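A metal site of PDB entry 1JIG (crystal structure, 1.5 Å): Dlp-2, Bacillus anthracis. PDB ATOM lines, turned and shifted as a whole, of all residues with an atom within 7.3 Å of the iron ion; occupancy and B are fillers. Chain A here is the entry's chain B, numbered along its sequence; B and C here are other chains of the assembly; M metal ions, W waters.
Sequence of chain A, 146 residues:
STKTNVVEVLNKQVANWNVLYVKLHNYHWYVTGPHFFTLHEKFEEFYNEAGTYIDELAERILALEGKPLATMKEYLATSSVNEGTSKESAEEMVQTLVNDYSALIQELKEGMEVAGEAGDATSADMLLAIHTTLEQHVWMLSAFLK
The indole nitrogen (NE1) of Trp 29 of chain B sits at hydrogen-bond distance from the side-chain carboxylate (OD1) of Asp 55 (2.8 Å). A ring nitrogen (ND1) of His 28 of chain B lies within hydrogen-bond range of the backbone carbonyl oxygen (O) of His 40 of chain B (2.6 Å). The side-chain carboxylate of Glu 59 sits close to a ring nitrogen (NE2) of His 40 of chain B, at 3.5 Å. The backbone carbonyl oxygen of Glu 59 lies close to the side-chain amide oxygen of Gln 136 of chain C (3.0 Å).
His 40 of chain B touches the iron ion (CE1 to FE, 3.97 Å). Four residues have an atom within 4 Å of the iron ion: Asp 55, Glu 59, His 28 of chain B and His 40 of chain B.
The iron ion is bound by OE1 of Glu 59 (2.0 Å), OD2 of Asp 55 (2.0 Å), NE2 of His 28 of chain B (2.1 Å) and water W1 (2.2 Å). Slightly farther from the iron ion lies the side-chain carboxylate (OD1) of Asp 55 (2.7 Å).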
ATOM      1  N   ASP A  55      16.969  27.021  -5.710  1.00  0.00           N
ATOM      2  CA  ASP A  55      15.745  27.734  -5.364  1.00  0.00           C
ATOM      3  C   ASP A  55      15.932  29.243  -5.447  1.00  0.00           C
ATOM      4  O   ASP A  55      15.032  29.943  -5.895  1.00  0.00           O
ATOM      5  CB  ASP A  55      15.277  27.335  -3.959  1.00  0.00           C
ATOM      6  CG  ASP A  55      13.841  27.709  -3.713  1.00  0.00           C
ATOM      7  OD1 ASP A  55      13.008  27.398  -4.596  1.00  0.00           O
ATOM      8  OD2 ASP A  55      13.524  28.303  -2.653  1.00  0.00           O
ATOM      9  N   GLU A  56      17.096  29.737  -5.032  1.00  0.00           N
ATOM     10  CA  GLU A  56      17.380  31.178  -5.065  1.00  0.00           C
ATOM     11  C   GLU A  56      17.376  31.700  -6.494  1.00  0.00           C
ATOM     12  O   GLU A  56      16.694  32.679  -6.801  1.00  0.00           O
ATOM     13  CB  GLU A  56      18.749  31.484  -4.448  1.00  0.00           C
ATOM     14  CG  GLU A  56      19.022  30.773  -3.137  1.00  0.00           C
ATOM     15  CD  GLU A  56      17.879  30.875  -2.161  1.00  0.00           C
ATOM     16  OE1 GLU A  56      17.819  30.042  -1.225  1.00  0.00           O
ATOM     17  OE2 GLU A  56      17.046  31.793  -2.305  1.00  0.00           O
ATOM     18  N   GLU A  59      13.905  31.527  -8.085  1.00  0.00           N
ATOM     19  CA  GLU A  59      12.981  32.527  -7.566  1.00  0.00           C
ATOM     20  C   GLU A  59      13.317  33.947  -8.015  1.00  0.00           C
ATOM     21  O   GLU A  59      12.456  34.830  -8.028  1.00  0.00           O
ATOM     22  CB  GLU A  59      12.871  32.397  -6.050  1.00  0.00           C
ATOM     23  CG  GLU A  59      11.972  31.225  -5.710  1.00  0.00           C
ATOM     24  CD  GLU A  59      11.880  30.887  -4.246  1.00  0.00           C
ATOM     25  OE1 GLU A  59      11.037  30.026  -3.903  1.00  0.00           O
ATOM     26  OE2 GLU A  59      12.651  31.451  -3.436  1.00  0.00           O
ATOM     27  N   HIS B  25       9.997  21.225  -7.122  1.00  0.00           N
ATOM     28  CA  HIS B  25      10.537  22.563  -7.288  1.00  0.00           C
ATOM     29  C   HIS B  25       9.708  23.283  -8.358  1.00  0.00           C
ATOM     30  O   HIS B  25       9.388  24.464  -8.229  1.00  0.00           O
ATOM     31  CB  HIS B  25      12.004  22.485  -7.688  1.00  0.00           C
ATOM     32  CG  HIS B  25      12.940  22.352  -6.532  1.00  0.00           C
ATOM     33  ND1 HIS B  25      13.531  23.437  -5.922  1.00  0.00           N
ATOM     34  CD2 HIS B  25      13.328  21.258  -5.832  1.00  0.00           C
ATOM     35  CE1 HIS B  25      14.252  23.020  -4.898  1.00  0.00           C
ATOM     36  NE2 HIS B  25      14.144  21.705  -4.813  1.00  0.00           N
ATOM     37  N   HIS B  28       6.508  24.312  -6.885  1.00  0.00           N
ATOM     38  CA  HIS B  28       6.838  25.310  -5.868  1.00  0.00           C
ATOM     39  C   HIS B  28       7.013  26.697  -6.529  1.00  0.00           C
ATOM     40  O   HIS B  28       6.571  27.716  -5.995  1.00  0.00           O
ATOM     41  CB  HIS B  28       8.140  24.862  -5.172  1.00  0.00           C
ATOM     42  CG  HIS B  28       8.712  25.856  -4.206  1.00  0.00           C
ATOM     43  ND1 HIS B  28       8.141  26.138  -2.992  1.00  0.00           N
ATOM     44  CD2 HIS B  28       9.861  26.577  -4.259  1.00  0.00           C
ATOM     45  CE1 HIS B  28       8.912  26.980  -2.322  1.00  0.00           C
ATOM     46  NE2 HIS B  28       9.964  27.261  -3.074  1.00  0.00           N
ATOM     47  N   TRP B  29       7.631  26.705  -7.701  1.00  0.00           N
ATOM     48  CA  TRP B  29       7.882  27.935  -8.457  1.00  0.00           C
ATOM     49  C   TRP B  29       6.721  28.432  -9.306  1.00  0.00           C
ATOM     50  O   TRP B  29       6.469  29.630  -9.388  1.00  0.00           O
ATOM     51  CB  TRP B  29       9.092  27.743  -9.393  1.00  0.00           C
ATOM     52  CG  TRP B  29      10.369  27.403  -8.698  1.00  0.00           C
ATOM     53  CD1 TRP B  29      10.767  27.833  -7.463  1.00  0.00           C
ATOM     54  CD2 TRP B  29      11.438  26.598  -9.215  1.00  0.00           C
ATOM     55  NE1 TRP B  29      12.022  27.338  -7.173  1.00  0.00           N
ATOM     56  CE2 TRP B  29      12.456  26.585  -8.229  1.00  0.00           C
ATOM     57  CE3 TRP B  29      11.634  25.889 -10.410  1.00  0.00           C
ATOM     58  CZ2 TRP B  29      13.663  25.889  -8.412  1.00  0.00           C
ATOM     59  CZ3 TRP B  29      12.832  25.195 -10.589  1.00  0.00           C
ATOM     60  CH2 TRP B  29      13.828  25.204  -9.586  1.00  0.00           C
ATOM     61  N   HIS B  40       2.960  26.908  -2.225  1.00  0.00           N
ATOM     62  CA  HIS B  40       4.359  27.273  -2.372  1.00  0.00           C
ATOM     63  C   HIS B  40       5.134  26.694  -1.175  1.00  0.00           C
ATOM     64  O   HIS B  40       6.142  26.011  -1.342  1.00  0.00           O
ATOM     65  CB  HIS B  40       4.506  28.799  -2.400  1.00  0.00           C
ATOM     66  CG  HIS B  40       5.913  29.285  -2.553  1.00  0.00           C
ATOM     67  ND1 HIS B  40       6.648  29.095  -3.703  1.00  0.00           N
ATOM     68  CD2 HIS B  40       6.708  29.985  -1.713  1.00  0.00           C
ATOM     69  CE1 HIS B  40       7.834  29.656  -3.575  1.00  0.00           C
ATOM     70  NE2 HIS B  40       7.899  30.202  -2.370  1.00  0.00           N
ATOM     71  N   GLU B  41       4.654  26.963   0.026  1.00  0.00           N
ATOM     72  CA  GLU B  41       5.323  26.460   1.224  1.00  0.00           C
ATOM     73  C   GLU B  41       5.238  24.951   1.341  1.00  0.00           C
ATOM     74  O   GLU B  41       6.242  24.283   1.630  1.00  0.00           O
ATOM     75  CB  GLU B  41       4.705  27.114   2.459  1.00  0.00           C
ATOM     76  CG  GLU B  41       5.211  28.523   2.703  1.00  0.00           C
ATOM     77  CD  GLU B  41       6.663  28.546   3.167  1.00  0.00           C
ATOM     78  OE1 GLU B  41       7.538  27.991   2.449  1.00  0.00           O
ATOM     79  OE2 GLU B  41       6.922  29.116   4.247  1.00  0.00           O
ATOM     80  N   GLU B  44       7.540  23.055  -0.804  1.00  0.00           N
ATOM     81  CA  GLU B  44       8.906  23.228  -0.347  1.00  0.00           C
ATOM     82  C   GLU B  44       9.206  22.181   0.725  1.00  0.00           C
ATOM     83  O   GLU B  44      10.281  21.584   0.734  1.00  0.00           O
ATOM     84  CB  GLU B  44       9.074  24.637   0.219  1.00  0.00           C
ATOM     85  CG  GLU B  44      10.428  25.266  -0.013  1.00  0.00           C
ATOM     86  CD  GLU B  44      11.422  24.940   1.072  1.00  0.00           C
ATOM     87  OE1 GLU B  44      12.385  25.715   1.233  1.00  0.00           O
ATOM     88  OE2 GLU B  44      11.230  23.903   1.756  1.00  0.00           O
ATOM     89  N   TYR B  47       9.637  18.878  -1.069  1.00  0.00           N
ATOM     90  CA  TYR B  47      10.911  18.703  -1.755  1.00  0.00           C
ATOM     91  C   TYR B  47      12.016  18.448  -0.723  1.00  0.00           C
ATOM     92  O   TYR B  47      12.977  17.734  -1.013  1.00  0.00           O
ATOM     93  CB  TYR B  47      11.226  19.936  -2.647  1.00  0.00           C
ATOM     94  CG  TYR B  47      12.262  20.902  -2.105  1.00  0.00           C
ATOM     95  CD1 TYR B  47      13.544  20.475  -1.782  1.00  0.00           C
ATOM     96  CD2 TYR B  47      11.958  22.263  -1.936  1.00  0.00           C
ATOM     97  CE1 TYR B  47      14.503  21.343  -1.303  1.00  0.00           C
ATOM     98  CE2 TYR B  47      12.923  23.149  -1.451  1.00  0.00           C
ATOM     99  CZ  TYR B  47      14.193  22.687  -1.140  1.00  0.00           C
ATOM    100  OH  TYR B  47      15.153  23.529  -0.650  1.00  0.00           O
ATOM    101  N   GLN C 136      10.847  40.218  -4.735  1.00  0.00           N
ATOM    102  CA  GLN C 136      10.390  38.889  -4.376  1.00  0.00           C
ATOM    103  C   GLN C 136       8.941  39.012  -3.927  1.00  0.00           C
ATOM    104  O   GLN C 136       8.094  38.202  -4.293  1.00  0.00           O
ATOM    105  CB  GLN C 136      11.233  38.301  -3.252  1.00  0.00           C
ATOM    106  CG  GLN C 136      12.584  37.811  -3.726  1.00  0.00           C
ATOM    107  CD  GLN C 136      12.462  36.669  -4.740  1.00  0.00           C
ATOM    108  OE1 GLN C 136      13.024  36.722  -5.827  1.00  0.00           O
ATOM    109  NE2 GLN C 136      11.711  35.637  -4.366  1.00  0.00           N
ATOM    110  N   TRP C 139       6.415  39.371  -6.890  1.00  0.00           N
ATOM    111  CA  TRP C 139       6.134  38.126  -7.609  1.00  0.00           C
ATOM    112  C   TRP C 139       5.116  37.282  -6.854  1.00  0.00           C
ATOM    113  O   TRP C 139       4.104  36.837  -7.426  1.00  0.00           O
ATOM    114  CB  TRP C 139       7.424  37.306  -7.830  1.00  0.00           C
ATOM    115  CG  TRP C 139       7.243  35.791  -7.705  1.00  0.00           C
ATOM    116  CD1 TRP C 139       6.332  35.013  -8.367  1.00  0.00           C
ATOM    117  CD2 TRP C 139       7.913  34.923  -6.795  1.00  0.00           C
ATOM    118  NE1 TRP C 139       6.390  33.712  -7.920  1.00  0.00           N
ATOM    119  CE2 TRP C 139       7.354  33.621  -6.950  1.00  0.00           C
ATOM    120  CE3 TRP C 139       8.934  35.099  -5.852  1.00  0.00           C
ATOM    121  CZ2 TRP C 139       7.774  32.533  -6.201  1.00  0.00           C
ATOM    122  CZ3 TRP C 139       9.355  33.998  -5.097  1.00  0.00           C
ATOM    123  CH2 TRP C 139       8.778  32.735  -5.286  1.00  0.00           C
HETATM  124 FE    FE M   1      11.549  28.559  -2.699  1.00  0.00          FE
HETATM  125  O   HOH W   1      11.388  29.016  -0.585  1.00  0.00           O
